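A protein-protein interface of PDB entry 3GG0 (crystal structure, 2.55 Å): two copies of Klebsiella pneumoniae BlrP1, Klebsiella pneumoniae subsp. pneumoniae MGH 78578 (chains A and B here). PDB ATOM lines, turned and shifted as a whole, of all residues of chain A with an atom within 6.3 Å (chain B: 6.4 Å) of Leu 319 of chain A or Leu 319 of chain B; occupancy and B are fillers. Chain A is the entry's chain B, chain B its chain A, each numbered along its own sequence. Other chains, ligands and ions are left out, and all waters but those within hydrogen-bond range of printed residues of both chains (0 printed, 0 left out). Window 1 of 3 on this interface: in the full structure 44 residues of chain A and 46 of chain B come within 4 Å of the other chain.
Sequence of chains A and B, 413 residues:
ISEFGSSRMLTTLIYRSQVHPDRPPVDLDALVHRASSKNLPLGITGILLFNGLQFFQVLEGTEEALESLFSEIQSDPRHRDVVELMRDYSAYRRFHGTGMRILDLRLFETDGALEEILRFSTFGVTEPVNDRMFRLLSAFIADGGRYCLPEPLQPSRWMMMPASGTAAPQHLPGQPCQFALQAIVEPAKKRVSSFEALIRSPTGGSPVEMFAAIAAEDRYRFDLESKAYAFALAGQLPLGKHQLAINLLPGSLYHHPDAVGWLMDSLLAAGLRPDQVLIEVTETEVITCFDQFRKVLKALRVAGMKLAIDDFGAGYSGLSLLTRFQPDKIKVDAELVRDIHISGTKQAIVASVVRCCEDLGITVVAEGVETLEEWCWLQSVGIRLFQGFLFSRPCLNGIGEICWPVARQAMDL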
ATOM      1  N   GLU A 283      -1.174   5.983  19.920  1.00  0.00           N
ATOM      2  CA  GLU A 283      -1.801   5.316  21.066  1.00  0.00           C
ATOM      3  C   GLU A 283      -0.787   4.698  22.034  1.00  0.00           C
ATOM      4  O   GLU A 283      -0.908   4.855  23.252  1.00  0.00           O
ATOM      5  CB  GLU A 283      -2.778   4.242  20.584  1.00  0.00           C
ATOM      6  CG  GLU A 283      -3.736   3.748  21.657  1.00  0.00           C
ATOM      7  CD  GLU A 283      -4.475   2.480  21.253  1.00  0.00           C
ATOM      8  OE1 GLU A 283      -4.000   1.771  20.337  1.00  0.00           O
ATOM      9  OE2 GLU A 283      -5.517   2.178  21.874  1.00  0.00           O
ATOM     10  N   PHE A 312      -5.042   3.858  16.806  1.00  0.00           N
ATOM     11  CA  PHE A 312      -5.766   3.099  17.819  1.00  0.00           C
ATOM     12  C   PHE A 312      -5.889   1.645  17.383  1.00  0.00           C
ATOM     13  O   PHE A 312      -6.353   1.357  16.283  1.00  0.00           O
ATOM     14  CB  PHE A 312      -7.157   3.704  18.038  1.00  0.00           C
ATOM     15  CG  PHE A 312      -7.853   3.212  19.280  1.00  0.00           C
ATOM     16  CD1 PHE A 312      -7.840   3.969  20.441  1.00  0.00           C
ATOM     17  CD2 PHE A 312      -8.547   2.009  19.277  1.00  0.00           C
ATOM     18  CE1 PHE A 312      -8.488   3.528  21.583  1.00  0.00           C
ATOM     19  CE2 PHE A 312      -9.190   1.562  20.415  1.00  0.00           C
ATOM     20  CZ  PHE A 312      -9.162   2.327  21.569  1.00  0.00           C
ATOM     21  N   SER A 317      -2.461  -1.423  23.148  1.00  0.00           N
ATOM     22  CA  SER A 317      -3.377  -0.500  23.841  1.00  0.00           C
ATOM     23  C   SER A 317      -4.815  -0.626  23.315  1.00  0.00           C
ATOM     24  O   SER A 317      -5.051  -1.218  22.256  1.00  0.00           O
ATOM     25  CB  SER A 317      -2.894   0.955  23.716  1.00  0.00           C
ATOM     26  OG  SER A 317      -1.532   1.032  23.315  1.00  0.00           O
ATOM     27  N   GLY A 318      -5.768  -0.061  24.056  1.00  0.00           N
ATOM     28  CA  GLY A 318      -7.184  -0.164  23.690  1.00  0.00           C
ATOM     29  C   GLY A 318      -8.106   0.764  24.469  1.00  0.00           C
ATOM     30  O   GLY A 318      -7.718   1.879  24.835  1.00  0.00           O
ATOM     31  N   LEU A 319      -9.329   0.292  24.727  1.00  0.00           N
ATOM     32  CA  LEU A 319     -10.393   1.127  25.315  1.00  0.00           C
ATOM     33  C   LEU A 319     -10.141   1.464  26.788  1.00  0.00           C
ATOM     34  O   LEU A 319     -10.768   2.369  27.342  1.00  0.00           O
ATOM     35  CB  LEU A 319     -11.766   0.447  25.164  1.00  0.00           C
ATOM     36  CG  LEU A 319     -12.278   0.110  23.755  1.00  0.00           C
ATOM     37  CD1 LEU A 319     -13.411  -0.903  23.824  1.00  0.00           C
ATOM     38  CD2 LEU A 319     -12.727   1.357  23.012  1.00  0.00           C
ATOM     39  N   SER A 320      -9.227   0.725  27.417  1.00  0.00           N
ATOM     40  CA  SER A 320      -8.866   0.954  28.819  1.00  0.00           C
ATOM     41  C   SER A 320      -8.239   2.332  29.014  1.00  0.00           C
ATOM     42  O   SER A 320      -8.308   2.911  30.104  1.00  0.00           O
ATOM     43  CB  SER A 320      -7.909  -0.139  29.306  1.00  0.00           C
ATOM     44  OG  SER A 320      -7.083  -0.609  28.251  1.00  0.00           O
ATOM     45  N   LEU A 321      -7.630   2.847  27.946  1.00  0.00           N
ATOM     46  CA  LEU A 321      -7.144   4.226  27.896  1.00  0.00           C
ATOM     47  C   LEU A 321      -8.286   5.239  28.073  1.00  0.00           C
ATOM     48  O   LEU A 321      -8.115   6.272  28.725  1.00  0.00           O
ATOM     49  CB  LEU A 321      -6.411   4.475  26.564  1.00  0.00           C
ATOM     50  CG  LEU A 321      -6.005   5.906  26.183  1.00  0.00           C
ATOM     51  CD1 LEU A 321      -4.879   6.414  27.078  1.00  0.00           C
ATOM     52  CD2 LEU A 321      -5.595   5.973  24.717  1.00  0.00           C
ATOM     53  N   LEU A 322      -9.454   4.920  27.513  1.00  0.00           N
ATOM     54  CA  LEU A 322     -10.595   5.845  27.510  1.00  0.00           C
ATOM     55  C   LEU A 322     -11.208   6.031  28.894  1.00  0.00           C
ATOM     56  O   LEU A 322     -12.014   6.939  29.105  1.00  0.00           O
ATOM     57  CB  LEU A 322     -11.667   5.390  26.516  1.00  0.00           C
ATOM     58  CG  LEU A 322     -11.216   5.108  25.079  1.00  0.00           C
ATOM     59  CD1 LEU A 322     -12.411   4.784  24.210  1.00  0.00           C
ATOM     60  CD2 LEU A 322     -10.436   6.286  24.502  1.00  0.00           C
ATOM     61  N   THR A 323     -10.826   5.168  29.830  1.00  0.00           N
ATOM     62  CA  THR A 323     -11.203   5.340  31.229  1.00  0.00           C
ATOM     63  C   THR A 323     -10.507   6.566  31.817  1.00  0.00           C
ATOM     64  O   THR A 323     -11.113   7.334  32.571  1.00  0.00           O
ATOM     65  CB  THR A 323     -10.838   4.098  32.077  1.00  0.00           C
ATOM     66  OG1 THR A 323     -11.017   2.904  31.298  1.00  0.00           O
ATOM     67  CG2 THR A 323     -11.711   4.029  33.335  1.00  0.00           C
ATOM     68  N   ARG A 324      -9.235   6.746  31.455  1.00  0.00           N
ATOM     69  CA  ARG A 324      -8.423   7.837  31.990  1.00  0.00           C
ATOM     70  C   ARG A 324      -8.925   9.184  31.471  1.00  0.00           C
ATOM     71  O   ARG A 324      -9.645   9.903  32.169  1.00  0.00           O
ATOM     72  CB  ARG A 324      -6.942   7.648  31.621  1.00  0.00           C
ATOM     73  CG  ARG A 324      -6.487   6.191  31.487  1.00  0.00           C
ATOM     74  CD  ARG A 324      -6.301   5.522  32.841  1.00  0.00           C
ATOM     75  NE  ARG A 324      -6.157   4.072  32.710  1.00  0.00           N
ATOM     76  CZ  ARG A 324      -6.241   3.213  33.724  1.00  0.00           C
ATOM     77  NH1 ARG A 324      -6.471   3.656  34.956  1.00  0.00           N
ATOM     78  NH2 ARG A 324      -6.098   1.912  33.509  1.00  0.00           N
ATOM     79  N   ILE A 330     -10.738   9.400  17.485  1.00  0.00           N
ATOM     80  CA  ILE A 330      -9.973   8.170  17.512  1.00  0.00           C
ATOM     81  C   ILE A 330      -9.727   7.666  16.093  1.00  0.00           C
ATOM     82  O   ILE A 330     -10.651   7.563  15.292  1.00  0.00           O
ATOM     83  CB  ILE A 330     -10.683   7.090  18.367  1.00  0.00           C
ATOM     84  CG1 ILE A 330     -10.394   7.331  19.854  1.00  0.00           C
ATOM     85  CG2 ILE A 330     -10.257   5.685  17.952  1.00  0.00           C
ATOM     86  CD1 ILE A 330     -11.033   6.322  20.780  1.00  0.00           C
ATOM     87  N   ALA A 348     -15.607  -7.718  14.934  1.00  0.00           N
ATOM     88  CA  ALA A 348     -16.137  -7.561  16.288  1.00  0.00           C
ATOM     89  C   ALA A 348     -15.424  -6.449  17.065  1.00  0.00           C
ATOM     90  O   ALA A 348     -16.068  -5.649  17.744  1.00  0.00           O
ATOM     91  CB  ALA A 348     -16.054  -8.875  17.042  1.00  0.00           C
ATOM     92  N   ILE A 349     -14.094  -6.414  16.959  1.00  0.00           N
ATOM     93  CA  ILE A 349     -13.287  -5.389  17.622  1.00  0.00           C
ATOM     94  C   ILE A 349     -13.674  -3.990  17.150  1.00  0.00           C
ATOM     95  O   ILE A 349     -13.936  -3.104  17.963  1.00  0.00           O
ATOM     96  CB  ILE A 349     -11.763  -5.610  17.384  1.00  0.00           C
ATOM     97  CG1 ILE A 349     -11.267  -6.838  18.151  1.00  0.00           C
ATOM     98  CG2 ILE A 349     -10.963  -4.370  17.792  1.00  0.00           C
ATOM     99  CD1 ILE A 349      -9.800  -7.189  17.879  1.00  0.00           C
ATOM    100  N   VAL A 350     -13.720  -3.804  15.835  1.00  0.00           N
ATOM    101  CA  VAL A 350     -13.984  -2.491  15.252  1.00  0.00           C
ATOM    102  C   VAL A 350     -15.417  -2.034  15.512  1.00  0.00           C
ATOM    103  O   VAL A 350     -15.647  -0.887  15.887  1.00  0.00           O
ATOM    104  CB  VAL A 350     -13.683  -2.468  13.726  1.00  0.00           C
ATOM    105  CG1 VAL A 350     -14.155  -1.158  13.096  1.00  0.00           C
ATOM    106  CG2 VAL A 350     -12.195  -2.681  13.478  1.00  0.00           C
ATOM    107  N   SER A 352     -17.155  -2.754  17.958  1.00  0.00           N
ATOM    108  CA  SER A 352     -17.242  -2.447  19.375  1.00  0.00           C
ATOM    109  C   SER A 352     -16.701  -1.053  19.661  1.00  0.00           C
ATOM    110  O   SER A 352     -17.314  -0.282  20.404  1.00  0.00           O
ATOM    111  CB  SER A 352     -16.475  -3.486  20.189  1.00  0.00           C
ATOM    112  OG  SER A 352     -16.902  -3.487  21.537  1.00  0.00           O
ATOM    113  N   VAL A 353     -15.557  -0.737  19.058  1.00  0.00           N
ATOM    114  CA  VAL A 353     -14.921   0.574  19.209  1.00  0.00           C
ATOM    115  C   VAL A 353     -15.816   1.683  18.662  1.00  0.00           C
ATOM    116  O   VAL A 353     -15.964   2.729  19.281  1.00  0.00           O
ATOM    117  CB  VAL A 353     -13.537   0.611  18.502  1.00  0.00           C
ATOM    118  CG1 VAL A 353     -13.022   2.028  18.390  1.00  0.00           C
ATOM    119  CG2 VAL A 353     -12.538  -0.266  19.244  1.00  0.00           C
ATOM    120  N   CYS A 356     -18.608   2.148  21.109  1.00  0.00           N
ATOM    121  CA  CYS A 356     -18.054   2.746  22.320  1.00  0.00           C
ATOM    122  C   CYS A 356     -17.867   4.249  22.158  1.00  0.00           C
ATOM    123  O   CYS A 356     -18.242   5.029  23.033  1.00  0.00           O
ATOM    124  CB  CYS A 356     -16.719   2.089  22.678  1.00  0.00           C
ATOM    125  SG  CYS A 356     -16.096   2.500  24.328  1.00  0.00           S
ATOM    126  N   CYS A 357     -17.308   4.648  21.023  1.00  0.00           N
ATOM    127  CA  CYS A 357     -17.007   6.047  20.768  1.00  0.00           C
ATOM    128  C   CYS A 357     -18.263   6.876  20.520  1.00  0.00           C
ATOM    129  O   CYS A 357     -18.292   8.074  20.810  1.00  0.00           O
ATOM    130  CB  CYS A 357     -16.057   6.171  19.596  1.00  0.00           C
ATOM    131  SG  CYS A 357     -14.422   5.522  19.926  1.00  0.00           S
ATOM    132  N   GLU B 283      -3.253  -9.025  32.539  1.00  0.00           N
ATOM    133  CA  GLU B 283      -3.192  -8.295  31.265  1.00  0.00           C
ATOM    134  C   GLU B 283      -1.822  -7.652  31.017  1.00  0.00           C
ATOM    135  O   GLU B 283      -1.320  -7.655  29.892  1.00  0.00           O
ATOM    136  CB  GLU B 283      -4.299  -7.226  31.230  1.00  0.00           C
ATOM    137  CG  GLU B 283      -4.445  -6.479  29.902  1.00  0.00           C
ATOM    138  CD  GLU B 283      -5.431  -5.310  29.991  1.00  0.00           C
ATOM    139  OE1 GLU B 283      -5.321  -4.502  30.936  1.00  0.00           O
ATOM    140  OE2 GLU B 283      -6.312  -5.200  29.115  1.00  0.00           O
ATOM    141  N   PHE B 312      -8.571  -7.495  33.082  1.00  0.00           N
ATOM    142  CA  PHE B 312      -8.702  -6.815  31.798  1.00  0.00           C
ATOM    143  C   PHE B 312      -9.302  -5.417  31.979  1.00  0.00           C
ATOM    144  O   PHE B 312     -10.277  -5.238  32.713  1.00  0.00           O
ATOM    145  CB  PHE B 312      -9.580  -7.650  30.864  1.00  0.00           C
ATOM    146  CG  PHE B 312      -9.676  -7.112  29.465  1.00  0.00           C
ATOM    147  CD1 PHE B 312      -8.680  -7.382  28.532  1.00  0.00           C
ATOM    148  CD2 PHE B 312     -10.783  -6.366  29.065  1.00  0.00           C
ATOM    149  CE1 PHE B 312      -8.772  -6.897  27.234  1.00  0.00           C
ATOM    150  CE2 PHE B 312     -10.882  -5.879  27.766  1.00  0.00           C
ATOM    151  CZ  PHE B 312      -9.877  -6.146  26.850  1.00  0.00           C
ATOM    152  N   GLY B 313      -8.712  -4.432  31.306  1.00  0.00           N
ATOM    153  CA  GLY B 313      -9.161  -3.046  31.413  1.00  0.00           C
ATOM    154  C   GLY B 313      -8.317  -2.223  32.372  1.00  0.00           C
ATOM    155  O   GLY B 313      -8.413  -0.993  32.404  1.00  0.00           O
ATOM    156  N   TYR B 316      -3.986  -1.108  30.662  1.00  0.00           N
ATOM    157  CA  TYR B 316      -3.845  -0.228  29.484  1.00  0.00           C
ATOM    158  C   TYR B 316      -3.961  -0.942  28.121  1.00  0.00           C
ATOM    159  O   TYR B 316      -4.648  -0.453  27.214  1.00  0.00           O
ATOM    160  CB  TYR B 316      -2.547   0.604  29.569  1.00  0.00           C
ATOM    161  CG  TYR B 316      -2.235   1.131  30.969  1.00  0.00           C
ATOM    162  CD1 TYR B 316      -3.133   1.968  31.641  1.00  0.00           C
ATOM    163  CD2 TYR B 316      -1.043   0.789  31.615  1.00  0.00           C
ATOM    164  CE1 TYR B 316      -2.852   2.446  32.923  1.00  0.00           C
ATOM    165  CE2 TYR B 316      -0.755   1.263  32.897  1.00  0.00           C
ATOM    166  CZ  TYR B 316      -1.664   2.089  33.543  1.00  0.00           C
ATOM    167  OH  TYR B 316      -1.385   2.560  34.807  1.00  0.00           O
ATOM    168  N   SER B 317      -3.287  -2.083  27.982  1.00  0.00           N
ATOM    169  CA  SER B 317      -3.322  -2.852  26.740  1.00  0.00           C
ATOM    170  C   SER B 317      -4.595  -3.689  26.620  1.00  0.00           C
ATOM    171  O   SER B 317      -4.590  -4.886  26.917  1.00  0.00           O
ATOM    172  CB  SER B 317      -2.097  -3.751  26.633  1.00  0.00           C
ATOM    173  OG  SER B 317      -2.113  -4.478  25.415  1.00  0.00           O
ATOM    174  N   GLY B 318      -5.665  -3.063  26.138  1.00  0.00           N
ATOM    175  CA  GLY B 318      -6.992  -3.667  26.164  1.00  0.00           C
ATOM    176  C   GLY B 318      -7.368  -4.491  24.940  1.00  0.00           C
ATOM    177  O   GLY B 318      -6.811  -5.563  24.702  1.00  0.00           O
ATOM    178  N   LEU B 319      -8.311  -3.971  24.158  1.00  0.00           N
ATOM    179  CA  LEU B 319      -9.134  -4.793  23.268  1.00  0.00           C
ATOM    180  C   LEU B 319      -8.441  -5.199  21.950  1.00  0.00           C
ATOM    181  O   LEU B 319      -8.924  -6.077  21.231  1.00  0.00           O
ATOM    182  CB  LEU B 319     -10.468  -4.086  22.993  1.00  0.00           C
ATOM    183  CG  LEU B 319     -11.685  -4.971  22.724  1.00  0.00           C
ATOM    184  CD1 LEU B 319     -12.820  -4.648  23.679  1.00  0.00           C
ATOM    185  CD2 LEU B 319     -12.128  -4.821  21.290  1.00  0.00           C
ATOM    186  N   SER B 320      -7.303  -4.576  21.655  1.00  0.00           N
ATOM    187  CA  SER B 320      -6.527  -4.920  20.460  1.00  0.00           C
ATOM    188  C   SER B 320      -5.717  -6.209  20.649  1.00  0.00           C
ATOM    189  O   SER B 320      -5.217  -6.787  19.679  1.00  0.00           O
ATOM    190  CB  SER B 320      -5.599  -3.771  20.079  1.00  0.00           C
ATOM    191  OG  SER B 320      -4.584  -3.594  21.052  1.00  0.00           O
ATOM    192  N   LEU B 321      -5.597  -6.649  21.902  1.00  0.00           N
ATOM    193  CA  LEU B 321      -4.881  -7.887  22.248  1.00  0.00           C
ATOM    194  C   LEU B 321      -5.505  -9.117  21.577  1.00  0.00           C
ATOM    195  O   LEU B 321      -4.820 -10.115  21.321  1.00  0.00           O
ATOM    196  CB  LEU B 321      -4.860  -8.072  23.773  1.00  0.00           C
ATOM    197  CG  LEU B 321      -4.133  -9.283  24.371  1.00  0.00           C
ATOM    198  CD1 LEU B 321      -2.638  -9.018  24.503  1.00  0.00           C
ATOM    199  CD2 LEU B 321      -4.730  -9.639  25.719  1.00  0.00           C
ATOM    200  N   LEU B 322      -6.799  -9.028  21.278  1.00  0.00           N
ATOM    201  CA  LEU B 322      -7.545 -10.138  20.690  1.00  0.00           C
ATOM    202  C   LEU B 322      -7.113 -10.436  19.250  1.00  0.00           C
ATOM    203  O   LEU B 322      -7.426 -11.492  18.708  1.00  0.00           O
ATOM    204  CB  LEU B 322      -9.049  -9.863  20.754  1.00  0.00           C
ATOM    205  CG  LEU B 322      -9.599  -9.458  22.129  1.00  0.00           C
ATOM    206  CD1 LEU B 322     -10.953  -8.760  22.004  1.00  0.00           C
ATOM    207  CD2 LEU B 322      -9.690 -10.658  23.057  1.00  0.00           C
ATOM    208  N   THR B 323      -6.392  -9.498  18.646  1.00  0.00           N
ATOM    209  CA  THR B 323      -5.791  -9.705  17.332  1.00  0.00           C
ATOM    210  C   THR B 323      -4.678 -10.751  17.411  1.00  0.00           C
ATOM    211  O   THR B 323      -4.477 -11.534  16.477  1.00  0.00           O
ATOM    212  CB  THR B 323      -5.212  -8.381  16.767  1.00  0.00           C
ATOM    213  OG1 THR B 323      -6.230  -7.374  16.779  1.00  0.00           O
ATOM    214  CG2 THR B 323      -4.710  -8.565  15.344  1.00  0.00           C
ATOM    215  N   LEU B 336     -13.207  -0.834  36.589  1.00  0.00           N
ATOM    216  CA  LEU B 336     -14.317  -0.619  35.667  1.00  0.00           C
ATOM    217  C   LEU B 336     -15.668  -0.916  36.323  1.00  0.00           C
ATOM    218  O   LEU B 336     -16.715  -0.492  35.828  1.00  0.00           O
ATOM    219  CB  LEU B 336     -14.141  -1.467  34.409  1.00  0.00           C
ATOM    220  CG  LEU B 336     -12.987  -1.087  33.477  1.00  0.00           C
ATOM    221  CD1 LEU B 336     -12.653  -2.238  32.555  1.00  0.00           C
ATOM    222  CD2 LEU B 336     -13.328   0.159  32.675  1.00  0.00           C
ATOM    223  N   ALA B 348     -20.016   2.504  29.185  1.00  0.00           N
ATOM    224  CA  ALA B 348     -19.759   2.378  27.752  1.00  0.00           C
ATOM    225  C   ALA B 348     -18.663   1.363  27.463  1.00  0.00           C
ATOM    226  O   ALA B 348     -18.847   0.457  26.644  1.00  0.00           O
ATOM    227  CB  ALA B 348     -19.401   3.723  27.159  1.00  0.00           C
ATOM    228  N   ILE B 349     -17.529   1.511  28.152  1.00  0.00           N
ATOM    229  CA  ILE B 349     -16.392   0.602  27.990  1.00  0.00           C
ATOM    230  C   ILE B 349     -16.771  -0.841  28.312  1.00  0.00           C
ATOM    231  O   ILE B 349     -16.590  -1.738  27.480  1.00  0.00           O
ATOM    232  CB  ILE B 349     -15.195   1.029  28.863  1.00  0.00           C
ATOM    233  CG1 ILE B 349     -14.653   2.378  28.394  1.00  0.00           C
ATOM    234  CG2 ILE B 349     -14.095  -0.014  28.808  1.00  0.00           C
ATOM    235  CD1 ILE B 349     -13.845   3.103  29.441  1.00  0.00           C
ATOM    236  N   SER B 352     -18.978  -2.423  25.848  1.00  0.00           N
ATOM    237  CA  SER B 352     -18.257  -2.729  24.619  1.00  0.00           C
ATOM    238  C   SER B 352     -17.367  -3.976  24.727  1.00  0.00           C
ATOM    239  O   SER B 352     -17.125  -4.651  23.729  1.00  0.00           O
ATOM    240  CB  SER B 352     -17.448  -1.523  24.151  1.00  0.00           C
ATOM    241  OG  SER B 352     -18.267  -0.646  23.393  1.00  0.00           O
ATOM    242  N   VAL B 353     -16.886  -4.275  25.934  1.00  0.00           N
ATOM    243  CA  VAL B 353     -16.193  -5.545  26.179  1.00  0.00           C
ATOM    244  C   VAL B 353     -17.185  -6.712  26.095  1.00  0.00           C
ATOM    245  O   VAL B 353     -16.889  -7.750  25.485  1.00  0.00           O
ATOM    246  CB  VAL B 353     -15.470  -5.557  27.554  1.00  0.00           C
ATOM    247  CG1 VAL B 353     -14.711  -6.864  27.751  1.00  0.00           C
ATOM    248  CG2 VAL B 353     -14.518  -4.381  27.660  1.00  0.00           C
ATOM    249  N   CYS B 356     -18.285  -7.243  22.316  1.00  0.00           N
ATOM    250  CA  CYS B 356     -17.150  -7.797  21.574  1.00  0.00           C
ATOM    251  C   CYS B 356     -16.907  -9.269  21.916  1.00  0.00           C
ATOM    252  O   CYS B 356     -16.683 -10.093  21.028  1.00  0.00           O
ATOM    253  CB  CYS B 356     -15.885  -6.988  21.840  1.00  0.00           C
ATOM    254  SG  CYS B 356     -14.430  -7.607  21.000  1.00  0.00           S
ATOM    255  N   CYS B 357     -16.970  -9.591  23.204  1.00  0.00           N
ATOM    256  CA  CYS B 357     -16.748 -10.954  23.666  1.00  0.00           C
ATOM    257  C   CYS B 357     -17.891 -11.896  23.291  1.00  0.00           C
ATOM    258  O   CYS B 357     -17.676 -13.091  23.098  1.00  0.00           O
ATOM    259  CB  CYS B 357     -16.527 -10.974  25.167  1.00  0.00           C
ATOM    260  SG  CYS B 357     -14.952 -10.290  25.687  1.00  0.00           S
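The backbone carbonyl oxygen (O) of Tyr 316 of chain B is in hydrogen-bond range of the backbone NH (N) of Gly 318 of chain A, 3.4 Å away.
The side-chain hydroxyl of Ser 320 of chain A sits at hydrogen-bond distance from the backbone carbonyl oxygen of Tyr 316 of chain B (2.7 Å).
The side-chain hydroxyl of Ser 320 of chain B sits at hydrogen-bond distance from the backbone carbonyl oxygen of Ser 317 of chain A, 2.7 Å away.
The backbone carbonyl oxygen (O) of Ser 352 of chain B sits at hydrogen-bond distance from the side-chain hydroxyl (OG) of Ser 352 of chain A, 2.5 Å away.
Gly 318 of chain A touches Leu 319 of chain B, but with the chains exchanged Leu 319 of chain A does not touch Gly 318 of chain B (4.8 Å).
Leu 319 of chain A touches Ile 349 of chain B, and with the chains exchanged Ile 349 of chain A touches Leu 319 of chain B.
Leu 322 of chain A touches Ile 349 of chain B, and with the chains exchanged Ile 349 of chain A touches Leu 322 of chain B.
Thr 323 of chain A touches Ile 349 of chain B, and with the chains exchanged Ile 349 of chain A touches Thr 323 of chain B.
15 positions are printed for both chains.
Of the 23 pairs that touch across the chains among the printed residues, 12 have their exchanged pair printed and touching as well.
Among the printed residues, pairs that only touch across the chains: Cys 356 of chain A with Ser 352 of chain B, Ser 320 of chain A with Gly 313 of chain B, Arg 324 of chain A with Tyr 316 of chain B, Thr 323 of chain A with Ile 349 of chain B, Ser 320 of chain A with Gly 318 of chain B, Ser 317 of chain A with Tyr 316 of chain B, Ile 349 of chain A with Leu 319 of chain B, Gly 318 of chain A with Gly 318 of chain B, Ser 352 of chain A with Cys 356 of chain B, Ser 317 of chain A with Ser 317 of chain B, Ile 349 of chain A with Thr 323 of chain B, Leu 319 of chain A with Leu 319 of chain B, Leu 319 of chain A with Ile 349 of chain B, Ser 317 of chain A with Gly 318 of chain B, Thr 323 of chain A with Leu 336 of chain B, Arg 324 of chain A with Gly 313 of chain B, Leu 322 of chain A with Ile 349 of chain B, Ile 349 of chain A with Leu 322 of chain B and Gly 318 of chain A with Leu 319 of chain B.
The side-chain carboxylate of Glu 283 of chain B lies within hydrogen-bond range of the backbone NH of Gly 313 of chain B (3.3 Å).
The backbone carbonyl oxygen (O) of Ser 320 of chain B is in hydrogen-bond range of the side-chain hydroxyl (OG1) of Thr 323 of chain B (3.1 Å).
The backbone carbonyl oxygen (O) of Ala 348 of chain B lies close to the side-chain hydroxyl (OG) of Ser 352 of chain B (3.5 Å).
OE2 of Glu 283 of chain A lies within hydrogen-bond range of N of Gly 318 of chain A.
O of Ser 320 of chain A sits at hydrogen-bond distance from OG1 of Thr 323 of chain A (3.0 Å).
Leu 319 of chain A touches just these residues of chain B: Leu 319 and Ile 349.
Of the printed residues of chain B, Arg 324 of chain A touches Gly 313 (3.9 Å) and Tyr 316 (3.3 Å).
Of the printed residues of chain B, Ile 349 of chain A touches Leu 319 (3.6 Å), Leu 322 (3.997 Å) and Thr 323 (3.7 Å).
Val 353 of chain A touches none of the printed residues of chain B.
Of the printed residues of chain A, Leu 319 of chain B touches Gly 318 (3.998 Å), Leu 319 (3.8 Å) and Ile 349 (3.6 Å).
The nearest residue of chain B that does not touch Leu 319 of chain A is Ser 352 of chain B (4.1 Å).
The nearest printed residue of chain B that does not touch Cys 356 of chain A is Ile 349 of chain B (4.1 Å).
Of the 18 printed residues of chain A, 10 touch a printed residue of chain B.
Among the printed residues, 23 pairs touch across the chains.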
